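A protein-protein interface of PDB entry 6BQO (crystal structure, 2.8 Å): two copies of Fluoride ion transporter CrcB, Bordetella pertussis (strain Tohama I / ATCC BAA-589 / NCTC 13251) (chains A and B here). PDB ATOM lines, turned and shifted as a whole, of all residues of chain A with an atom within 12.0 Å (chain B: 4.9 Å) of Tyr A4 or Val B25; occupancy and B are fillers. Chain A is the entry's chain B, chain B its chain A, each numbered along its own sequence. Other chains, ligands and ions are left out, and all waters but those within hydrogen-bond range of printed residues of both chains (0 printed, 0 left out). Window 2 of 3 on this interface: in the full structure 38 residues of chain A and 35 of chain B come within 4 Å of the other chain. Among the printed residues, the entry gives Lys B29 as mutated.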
ATOM      1  N   MET A   1      23.051  -9.787  14.644  1.00  0.00           N
ATOM      2  CA  MET A   1      21.875 -10.049  13.821  1.00  0.00           C
ATOM      3  C   MET A   1      21.497  -8.818  13.001  1.00  0.00           C
ATOM      4  O   MET A   1      22.047  -7.733  13.199  1.00  0.00           O
ATOM      5  CB  MET A   1      20.692 -10.482  14.692  1.00  0.00           C
ATOM      6  CG  MET A   1      20.956 -11.709  15.556  1.00  0.00           C
ATOM      7  SD  MET A   1      21.263 -13.217  14.612  1.00  0.00           S
ATOM      8  CE  MET A   1      19.700 -13.420  13.761  1.00  0.00           C
ATOM      9  N   LEU A   2      20.562  -8.998  12.073  1.00  0.00           N
ATOM     10  CA  LEU A   2      20.031  -7.916  11.261  1.00  0.00           C
ATOM     11  C   LEU A   2      18.516  -7.867  11.409  1.00  0.00           C
ATOM     12  O   LEU A   2      17.888  -8.815  11.889  1.00  0.00           O
ATOM     13  CB  LEU A   2      20.412  -8.080   9.781  1.00  0.00           C
ATOM     14  CG  LEU A   2      21.901  -7.980   9.441  1.00  0.00           C
ATOM     15  CD1 LEU A   2      22.139  -8.233   7.959  1.00  0.00           C
ATOM     16  CD2 LEU A   2      22.455  -6.624   9.852  1.00  0.00           C
ATOM     17  N   THR A   3      17.934  -6.744  10.995  1.00  0.00           N
ATOM     18  CA  THR A   3      16.492  -6.571  11.109  1.00  0.00           C
ATOM     19  C   THR A   3      15.765  -7.626  10.283  1.00  0.00           C
ATOM     20  O   THR A   3      16.214  -8.010   9.200  1.00  0.00           O
ATOM     21  CB  THR A   3      16.083  -5.170  10.649  1.00  0.00           C
ATOM     22  OG1 THR A   3      16.855  -4.190  11.354  1.00  0.00           O
ATOM     23  CG2 THR A   3      14.605  -4.932  10.922  1.00  0.00           C
ATOM     24  N   TYR A   4      14.632  -8.096  10.804  1.00  0.00           N
ATOM     25  CA  TYR A   4      13.822  -9.129  10.166  1.00  0.00           C
ATOM     26  C   TYR A   4      14.430 -10.519  10.304  1.00  0.00           C
ATOM     27  O   TYR A   4      14.133 -11.410   9.500  1.00  0.00           O
ATOM     28  CB  TYR A   4      13.580  -8.820   8.685  1.00  0.00           C
ATOM     29  CG  TYR A   4      12.657  -7.648   8.432  1.00  0.00           C
ATOM     30  CD1 TYR A   4      12.092  -6.941   9.484  1.00  0.00           C
ATOM     31  CD2 TYR A   4      12.337  -7.261   7.136  1.00  0.00           C
ATOM     32  CE1 TYR A   4      11.244  -5.875   9.252  1.00  0.00           C
ATOM     33  CE2 TYR A   4      11.491  -6.198   6.895  1.00  0.00           C
ATOM     34  CZ  TYR A   4      10.946  -5.509   7.956  1.00  0.00           C
ATOM     35  OH  TYR A   4      10.101  -4.448   7.718  1.00  0.00           O
ATOM     36  N   ALA A   5      15.278 -10.728  11.306  1.00  0.00           N
ATOM     37  CA  ALA A   5      15.853 -12.043  11.529  1.00  0.00           C
ATOM     38  C   ALA A   5      14.808 -12.982  12.131  1.00  0.00           C
ATOM     39  O   ALA A   5      13.941 -12.553  12.899  1.00  0.00           O
ATOM     40  CB  ALA A   5      17.062 -11.952  12.454  1.00  0.00           C
ATOM     41  N   PRO A   6      14.870 -14.273  11.799  1.00  0.00           N
ATOM     42  CA  PRO A   6      13.901 -15.218  12.374  1.00  0.00           C
ATOM     43  C   PRO A   6      13.911 -15.239  13.892  1.00  0.00           C
ATOM     44  O   PRO A   6      12.852 -15.428  14.505  1.00  0.00           O
ATOM     45  CB  PRO A   6      14.337 -16.568  11.784  1.00  0.00           C
ATOM     46  CG  PRO A   6      15.769 -16.369  11.384  1.00  0.00           C
ATOM     47  CD  PRO A   6      15.854 -14.944  10.935  1.00  0.00           C
ATOM     48  N   LEU A   7      15.073 -15.050  14.522  1.00  0.00           N
ATOM     49  CA  LEU A   7      15.133 -15.028  15.980  1.00  0.00           C
ATOM     50  C   LEU A   7      14.442 -13.804  16.566  1.00  0.00           C
ATOM     51  O   LEU A   7      14.118 -13.803  17.759  1.00  0.00           O
ATOM     52  CB  LEU A   7      16.591 -15.090  16.446  1.00  0.00           C
ATOM     53  CG  LEU A   7      16.870 -15.225  17.947  1.00  0.00           C
ATOM     54  CD1 LEU A   7      18.131 -16.048  18.182  1.00  0.00           C
ATOM     55  CD2 LEU A   7      16.999 -13.861  18.613  1.00  0.00           C
ATOM     56  N   ASN A   8      14.209 -12.765  15.760  1.00  0.00           N
ATOM     57  CA  ASN A   8      13.497 -11.591  16.253  1.00  0.00           C
ATOM     58  C   ASN A   8      12.010 -11.879  16.411  1.00  0.00           C
ATOM     59  O   ASN A   8      11.420 -11.595  17.460  1.00  0.00           O
ATOM     60  CB  ASN A   8      13.719 -10.404  15.315  1.00  0.00           C
ATOM     61  CG  ASN A   8      15.125  -9.841  15.407  1.00  0.00           C
ATOM     62  OD1 ASN A   8      15.848 -10.096  16.371  1.00  0.00           O
ATOM     63  ND2 ASN A   8      15.516  -9.059  14.407  1.00  0.00           N
ATOM     64  N   PHE A   9      11.383 -12.438  15.372  1.00  0.00           N
ATOM     65  CA  PHE A   9       9.974 -12.801  15.468  1.00  0.00           C
ATOM     66  C   PHE A   9       9.724 -13.711  16.661  1.00  0.00           C
ATOM     67  O   PHE A   9       8.701 -13.590  17.345  1.00  0.00           O
ATOM     68  CB  PHE A   9       9.518 -13.472  14.172  1.00  0.00           C
ATOM     69  CG  PHE A   9       9.577 -12.575  12.968  1.00  0.00           C
ATOM     70  CD1 PHE A   9      10.773 -12.349  12.311  1.00  0.00           C
ATOM     71  CD2 PHE A   9       8.433 -11.963  12.490  1.00  0.00           C
ATOM     72  CE1 PHE A   9      10.827 -11.524  11.202  1.00  0.00           C
ATOM     73  CE2 PHE A   9       8.481 -11.139  11.382  1.00  0.00           C
ATOM     74  CZ  PHE A   9       9.679 -10.920  10.738  1.00  0.00           C
ATOM     75  N   ILE A  10      10.654 -14.628  16.931  1.00  0.00           N
ATOM     76  CA  ILE A  10      10.530 -15.496  18.100  1.00  0.00           C
ATOM     77  C   ILE A  10      10.463 -14.659  19.371  1.00  0.00           C
ATOM     78  O   ILE A  10       9.545 -14.806  20.188  1.00  0.00           O
ATOM     79  CB  ILE A  10      11.697 -16.500  18.144  1.00  0.00           C
ATOM     80  CG1 ILE A  10      11.851 -17.196  16.790  1.00  0.00           C
ATOM     81  CG2 ILE A  10      11.491 -17.515  19.258  1.00  0.00           C
ATOM     82  CD1 ILE A  10      10.578 -17.832  16.278  1.00  0.00           C
ATOM     83  N   ALA A  11      11.434 -13.757  19.551  1.00  0.00           N
ATOM     84  CA  ALA A  11      11.479 -12.941  20.759  1.00  0.00           C
ATOM     85  C   ALA A  11      10.261 -12.034  20.877  1.00  0.00           C
ATOM     86  O   ALA A  11       9.853 -11.687  21.991  1.00  0.00           O
ATOM     87  CB  ALA A  11      12.763 -12.112  20.783  1.00  0.00           C
ATOM     88  N   ILE A  12       9.672 -11.633  19.751  1.00  0.00           N
ATOM     89  CA  ILE A  12       8.467 -10.813  19.802  1.00  0.00           C
ATOM     90  C   ILE A  12       7.249 -11.668  20.125  1.00  0.00           C
ATOM     91  O   ILE A  12       6.439 -11.320  20.992  1.00  0.00           O
ATOM     92  CB  ILE A  12       8.286 -10.045  18.481  1.00  0.00           C
ATOM     93  CG1 ILE A  12       9.406  -9.020  18.307  1.00  0.00           C
ATOM     94  CG2 ILE A  12       6.921  -9.373  18.436  1.00  0.00           C
ATOM     95  CD1 ILE A  12       9.220  -8.114  17.114  1.00  0.00           C
ATOM     96  N   GLY A  13       7.102 -12.802  19.436  1.00  0.00           N
ATOM     97  CA  GLY A  13       5.971 -13.676  19.705  1.00  0.00           C
ATOM     98  C   GLY A  13       5.944 -14.166  21.139  1.00  0.00           C
ATOM     99  O   GLY A  13       4.911 -14.107  21.811  1.00  0.00           O
ATOM    100  N   ALA A  16       5.185 -11.152  23.405  1.00  0.00           N
ATOM    101  CA  ALA A  16       3.796 -10.734  23.252  1.00  0.00           C
ATOM    102  C   ALA A  16       2.845 -11.754  23.863  1.00  0.00           C
ATOM    103  O   ALA A  16       1.821 -11.386  24.452  1.00  0.00           O
ATOM    104  CB  ALA A  16       3.472 -10.514  21.774  1.00  0.00           C
ATOM    105  N   ALA A  65      20.037  -6.915  20.697  1.00  0.00           N
ATOM    106  CA  ALA A  65      18.816  -6.240  20.278  1.00  0.00           C
ATOM    107  C   ALA A  65      17.556  -7.010  20.653  1.00  0.00           C
ATOM    108  O   ALA A  65      16.467  -6.425  20.640  1.00  0.00           O
ATOM    109  CB  ALA A  65      18.839  -5.996  18.769  1.00  0.00           C
ATOM    110  N   TRP A  66      17.665  -8.301  20.979  1.00  0.00           N
ATOM    111  CA  TRP A  66      16.466  -9.077  21.272  1.00  0.00           C
ATOM    112  C   TRP A  66      15.901  -8.785  22.656  1.00  0.00           C
ATOM    113  O   TRP A  66      14.721  -9.064  22.899  1.00  0.00           O
ATOM    114  CB  TRP A  66      16.729 -10.583  21.112  1.00  0.00           C
ATOM    115  CG  TRP A  66      17.833 -11.152  21.957  1.00  0.00           C
ATOM    116  CD1 TRP A  66      19.138 -11.317  21.595  1.00  0.00           C
ATOM    117  CD2 TRP A  66      17.721 -11.660  23.293  1.00  0.00           C
ATOM    118  NE1 TRP A  66      19.848 -11.884  22.627  1.00  0.00           N
ATOM    119  CE2 TRP A  66      19.002 -12.103  23.681  1.00  0.00           C
ATOM    120  CE3 TRP A  66      16.663 -11.776  24.202  1.00  0.00           C
ATOM    121  CZ2 TRP A  66      19.254 -12.653  24.938  1.00  0.00           C
ATOM    122  CZ3 TRP A  66      16.918 -12.322  25.451  1.00  0.00           C
ATOM    123  CH2 TRP A  66      18.203 -12.753  25.806  1.00  0.00           C
ATOM    124  N   ARG A  68      15.357  -5.826  23.594  1.00  0.00           N
ATOM    125  CA  ARG A  68      14.400  -4.771  23.291  1.00  0.00           C
ATOM    126  C   ARG A  68      13.167  -5.325  22.589  1.00  0.00           C
ATOM    127  O   ARG A  68      12.039  -4.938  22.914  1.00  0.00           O
ATOM    128  CB  ARG A  68      15.066  -3.690  22.440  1.00  0.00           C
ATOM    129  CG  ARG A  68      14.121  -2.610  21.949  1.00  0.00           C
ATOM    130  CD  ARG A  68      14.873  -1.588  21.123  1.00  0.00           C
ATOM    131  NE  ARG A  68      15.786  -2.238  20.190  1.00  0.00           N
ATOM    132  CZ  ARG A  68      15.469  -2.573  18.946  1.00  0.00           C
ATOM    133  NH1 ARG A  68      14.258  -2.310  18.476  1.00  0.00           N
ATOM    134  NH2 ARG A  68      16.363  -3.165  18.169  1.00  0.00           N
ATOM    135  N   LEU A  69      13.361  -6.235  21.635  1.00  0.00           N
ATOM    136  CA  LEU A  69      12.229  -6.798  20.908  1.00  0.00           C
ATOM    137  C   LEU A  69      11.389  -7.703  21.801  1.00  0.00           C
ATOM    138  O   LEU A  69      10.160  -7.749  21.669  1.00  0.00           O
ATOM    139  CB  LEU A  69      12.731  -7.562  19.682  1.00  0.00           C
ATOM    140  CG  LEU A  69      13.516  -6.721  18.677  1.00  0.00           C
ATOM    141  CD1 LEU A  69      14.121  -7.601  17.595  1.00  0.00           C
ATOM    142  CD2 LEU A  69      12.621  -5.652  18.068  1.00  0.00           C
ATOM    143  N   VAL A  72      10.234  -5.123  25.238  1.00  0.00           N
ATOM    144  CA  VAL A  72       9.436  -3.946  24.912  1.00  0.00           C
ATOM    145  C   VAL A  72       8.440  -4.282  23.811  1.00  0.00           C
ATOM    146  O   VAL A  72       7.227  -4.300  24.043  1.00  0.00           O
ATOM    147  CB  VAL A  72      10.328  -2.759  24.503  1.00  0.00           C
ATOM    148  CG1 VAL A  72       9.472  -1.593  24.038  1.00  0.00           C
ATOM    149  CG2 VAL A  72      11.219  -2.343  25.665  1.00  0.00           C
ATOM    150  N   THR A  73       8.946  -4.544  22.604  1.00  0.00           N
ATOM    151  CA  THR A  73       8.057  -4.856  21.489  1.00  0.00           C
ATOM    152  C   THR A  73       7.235  -6.109  21.762  1.00  0.00           C
ATOM    153  O   THR A  73       6.097  -6.218  21.292  1.00  0.00           O
ATOM    154  CB  THR A  73       8.865  -5.019  20.202  1.00  0.00           C
ATOM    155  OG1 THR A  73       9.593  -3.813  19.939  1.00  0.00           O
ATOM    156  CG2 THR A  73       7.945  -5.311  19.027  1.00  0.00           C
ATOM    157  N   GLY A  74       7.785  -7.056  22.517  1.00  0.00           N
ATOM    158  CA  GLY A  74       7.068  -8.273  22.837  1.00  0.00           C
ATOM    159  C   GLY A  74       6.211  -8.155  24.080  1.00  0.00           C
ATOM    160  O   GLY A  74       5.002  -7.919  23.991  1.00  0.00           O
ATOM    161  N   GLY A  77       4.444  -4.957  24.749  1.00  0.00           N
ATOM    162  CA  GLY A  77       3.531  -4.766  23.638  1.00  0.00           C
ATOM    163  C   GLY A  77       2.279  -5.612  23.710  1.00  0.00           C
ATOM    164  O   GLY A  77       1.283  -5.282  23.060  1.00  0.00           O
ATOM    165  N   TRP B  21       3.662  -8.748  15.719  1.00  0.00           N
ATOM    166  CA  TRP B  21       4.455  -8.691  14.494  1.00  0.00           C
ATOM    167  C   TRP B  21       3.976  -7.569  13.582  1.00  0.00           C
ATOM    168  O   TRP B  21       4.780  -6.773  13.083  1.00  0.00           O
ATOM    169  CB  TRP B  21       4.401 -10.034  13.764  1.00  0.00           C
ATOM    170  CG  TRP B  21       5.187 -11.110  14.439  1.00  0.00           C
ATOM    171  CD1 TRP B  21       6.072 -10.958  15.467  1.00  0.00           C
ATOM    172  CD2 TRP B  21       5.156 -12.509  14.139  1.00  0.00           C
ATOM    173  NE1 TRP B  21       6.595 -12.177  15.825  1.00  0.00           N
ATOM    174  CE2 TRP B  21       6.048 -13.146  15.025  1.00  0.00           C
ATOM    175  CE3 TRP B  21       4.460 -13.286  13.208  1.00  0.00           C
ATOM    176  CZ2 TRP B  21       6.263 -14.522  15.006  1.00  0.00           C
ATOM    177  CZ3 TRP B  21       4.676 -14.652  13.191  1.00  0.00           C
ATOM    178  CH2 TRP B  21       5.569 -15.256  14.084  1.00  0.00           C
ATOM    179  N   LEU B  22       2.664  -7.485  13.357  1.00  0.00           N
ATOM    180  CA  LEU B  22       2.143  -6.442  12.480  1.00  0.00           C
ATOM    181  C   LEU B  22       2.441  -5.054  13.038  1.00  0.00           C
ATOM    182  O   LEU B  22       2.794  -4.138  12.287  1.00  0.00           O
ATOM    183  CB  LEU B  22       0.642  -6.631  12.266  1.00  0.00           C
ATOM    184  CG  LEU B  22      -0.064  -5.529  11.473  1.00  0.00           C
ATOM    185  CD1 LEU B  22       0.599  -5.318  10.120  1.00  0.00           C
ATOM    186  CD2 LEU B  22      -1.540  -5.854  11.306  1.00  0.00           C
ATOM    187  N   ARG B  23       2.302  -4.879  14.355  1.00  0.00           N
ATOM    188  CA  ARG B  23       2.615  -3.590  14.963  1.00  0.00           C
ATOM    189  C   ARG B  23       4.090  -3.256  14.796  1.00  0.00           C
ATOM    190  O   ARG B  23       4.448  -2.125  14.451  1.00  0.00           O
ATOM    191  CB  ARG B  23       2.240  -3.602  16.445  1.00  0.00           C
ATOM    192  CG  ARG B  23       2.404  -2.263  17.142  1.00  0.00           C
ATOM    193  CD  ARG B  23       2.248  -2.390  18.654  1.00  0.00           C
ATOM    194  NE  ARG B  23       3.425  -2.986  19.286  1.00  0.00           N
ATOM    195  CZ  ARG B  23       3.453  -4.193  19.842  1.00  0.00           C
ATOM    196  NH1 ARG B  23       2.365  -4.947  19.858  1.00  0.00           N
ATOM    197  NH2 ARG B  23       4.572  -4.643  20.392  1.00  0.00           N
ATOM    198  N   TRP B  24       4.957  -4.237  15.039  1.00  0.00           N
ATOM    199  CA  TRP B  24       6.391  -4.036  14.868  1.00  0.00           C
ATOM    200  C   TRP B  24       6.716  -3.539  13.463  1.00  0.00           C
ATOM    201  O   TRP B  24       7.354  -2.494  13.295  1.00  0.00           O
ATOM    202  CB  TRP B  24       7.117  -5.346  15.168  1.00  0.00           C
ATOM    203  CG  TRP B  24       8.597  -5.294  15.038  1.00  0.00           C
ATOM    204  CD1 TRP B  24       9.429  -4.298  15.456  1.00  0.00           C
ATOM    205  CD2 TRP B  24       9.429  -6.293  14.445  1.00  0.00           C
ATOM    206  NE1 TRP B  24      10.732  -4.619  15.162  1.00  0.00           N
ATOM    207  CE2 TRP B  24      10.758  -5.840  14.540  1.00  0.00           C
ATOM    208  CE3 TRP B  24       9.177  -7.530  13.845  1.00  0.00           C
ATOM    209  CZ2 TRP B  24      11.832  -6.581  14.054  1.00  0.00           C
ATOM    210  CZ3 TRP B  24      10.243  -8.263  13.366  1.00  0.00           C
ATOM    211  CH2 TRP B  24      11.555  -7.787  13.472  1.00  0.00           C
ATOM    212  N   VAL B  25       6.268  -4.270  12.440  1.00  0.00           N
ATOM    213  CA  VAL B  25       6.586  -3.898  11.063  1.00  0.00           C
ATOM    214  C   VAL B  25       6.006  -2.531  10.728  1.00  0.00           C
ATOM    215  O   VAL B  25       6.619  -1.744   9.996  1.00  0.00           O
ATOM    216  CB  VAL B  25       6.088  -4.982  10.089  1.00  0.00           C
ATOM    217  CG1 VAL B  25       6.348  -4.563   8.650  1.00  0.00           C
ATOM    218  CG2 VAL B  25       6.763  -6.311  10.391  1.00  0.00           C
ATOM    219  N   LEU B  26       4.818  -2.223  11.250  1.00  0.00           N
ATOM    220  CA  LEU B  26       4.247  -0.898  11.028  1.00  0.00           C
ATOM    221  C   LEU B  26       5.144   0.188  11.606  1.00  0.00           C
ATOM    222  O   LEU B  26       5.360   1.229  10.975  1.00  0.00           O
ATOM    223  CB  LEU B  26       2.845  -0.819  11.630  1.00  0.00           C
ATOM    224  CG  LEU B  26       1.754  -1.573  10.873  1.00  0.00           C
ATOM    225  CD1 LEU B  26       0.432  -1.492  11.617  1.00  0.00           C
ATOM    226  CD2 LEU B  26       1.614  -1.021   9.463  1.00  0.00           C
ATOM    227  N   GLY B  27       5.678  -0.037  12.808  1.00  0.00           N
ATOM    228  CA  GLY B  27       6.583   0.938  13.393  1.00  0.00           C
ATOM    229  C   GLY B  27       7.862   1.096  12.592  1.00  0.00           C
ATOM    230  O   GLY B  27       8.341   2.213  12.381  1.00  0.00           O
ATOM    231  N   LEU B  28       8.429  -0.019  12.131  1.00  0.00           N
ATOM    232  CA  LEU B  28       9.654   0.039  11.341  1.00  0.00           C
ATOM    233  C   LEU B  28       9.454   0.866  10.077  1.00  0.00           C
ATOM    234  O   LEU B  28      10.192   1.824   9.820  1.00  0.00           O
ATOM    235  CB  LEU B  28      10.121  -1.374  10.992  1.00  0.00           C
ATOM    236  CG  LEU B  28      10.657  -2.230  12.141  1.00  0.00           C
ATOM    237  CD1 LEU B  28      11.038  -3.619  11.652  1.00  0.00           C
ATOM    238  CD2 LEU B  28      11.846  -1.553  12.807  1.00  0.00           C
ATOM    239  N   LYS B  29       8.446   0.515   9.277  1.00  0.00           N
ATOM    240  CA  LYS B  29       8.297   1.115   7.957  1.00  0.00           C
ATOM    241  C   LYS B  29       7.561   2.447   7.975  1.00  0.00           C
ATOM    242  O   LYS B  29       7.696   3.220   7.021  1.00  0.00           O
ATOM    243  CB  LYS B  29       7.563   0.156   7.017  1.00  0.00           C
ATOM    244  CG  LYS B  29       7.846   0.415   5.542  1.00  0.00           C
ATOM    245  CD  LYS B  29       6.647   0.088   4.662  1.00  0.00           C
ATOM    246  CE  LYS B  29       5.566   1.154   4.781  1.00  0.00           C
ATOM    247  NZ  LYS B  29       4.438   0.920   3.834  1.00  0.00           N
ATOM    248  N   LEU B  30       6.793   2.738   9.022  1.00  0.00           N
ATOM    249  CA  LEU B  30       5.911   3.901   9.032  1.00  0.00           C
ATOM    250  C   LEU B  30       6.331   4.999   9.997  1.00  0.00           C
ATOM    251  O   LEU B  30       6.156   6.178   9.683  1.00  0.00           O
ATOM    252  CB  LEU B  30       4.478   3.470   9.364  1.00  0.00           C
ATOM    253  CG  LEU B  30       3.764   2.650   8.290  1.00  0.00           C
ATOM    254  CD1 LEU B  30       2.330   2.353   8.699  1.00  0.00           C
ATOM    255  CD2 LEU B  30       3.804   3.375   6.954  1.00  0.00           C
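The side-chain amide nitrogen (ND2) of Asn A8 is in hydrogen-bond range of the backbone carbonyl oxygen (O) of Leu A2 (3.5 Å). O of Arg A68 is in hydrogen-bond range of N of Thr A73 (3.1 Å). The backbone NH (N) of Gly A74 lies within hydrogen-bond range of the backbone carbonyl oxygen (O) of Leu A69, at 2.6 Å. N of Gly A77 sits at hydrogen-bond distance from O of Val A72 (2.9 Å).
Printed residues of chain B within 4 Å of Tyr A4: Val B25 (3.9 Å) and Leu B28 (3.3 Å). Leu B26 touches none of the printed residues of chain A. Leu B28 touches just these residues of chain A: Thr A3 and Tyr A4. Lys B29 touches none of the printed residues of chain A. No residue of chain A comes within 4 Å of Leu B30. Of the printed residues of chain B, Phe A9 touches Trp B21 and Trp B24. Of the printed residues of chain B, Thr A3 touches Leu B28. Printed residues of chain B within 4 Å of Thr A73: Arg B23 and Trp B24. Of the printed residues of chain B, Gly A13 touches Trp B21. The nearest printed residue of chain B that does not touch Ile A12 is Arg B23 (5.6 Å).
Of the 10 printed residues of chain B, 5 touch a printed residue of chain A. Hydrophobic or aromatic side chains of chain B that line the printed part of chain A: Trp B21, Trp B24, Val B25 and Leu B28. Printed residues of chain A that touch a printed residue of chain B: Thr A3, Tyr A4, Asn A8, Phe A9, Ile A12, Gly A13, Leu A69, Thr A73 and Gly A77. Among the printed residues, 13 pairs touch across the chains. Among the printed residues, no Asp or Glu carboxylate lies within 4 Å of a Lys or Arg side-chain nitrogen of the other chain.
Among the printed residues, merely in contact across the chains: Thr A3 with Leu B28, Tyr A4 with Val B25, Tyr A4 with Leu B28, Asn A8 with Trp B24, Phe A9 with Trp B24, Ile A12 with Trp B21, Ile A12 with Trp B24, Gly A13 with Trp B21, Leu A69 with Trp B24 and Thr A73 with Trp B24.
No position is printed for both chains.
The indole nitrogen (NE1) of Trp B21 is in hydrogen-bond range of the backbone carbonyl oxygen (O) of Phe A9. The backbone carbonyl oxygen (O) of Gly A77 sits at hydrogen-bond distance from the guanidinium group (NH1) of Arg B23. The backbone carbonyl oxygen (O) of Thr A73 lies close to the guanidinium group (NH2) of Arg B23 (2.4 Å).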
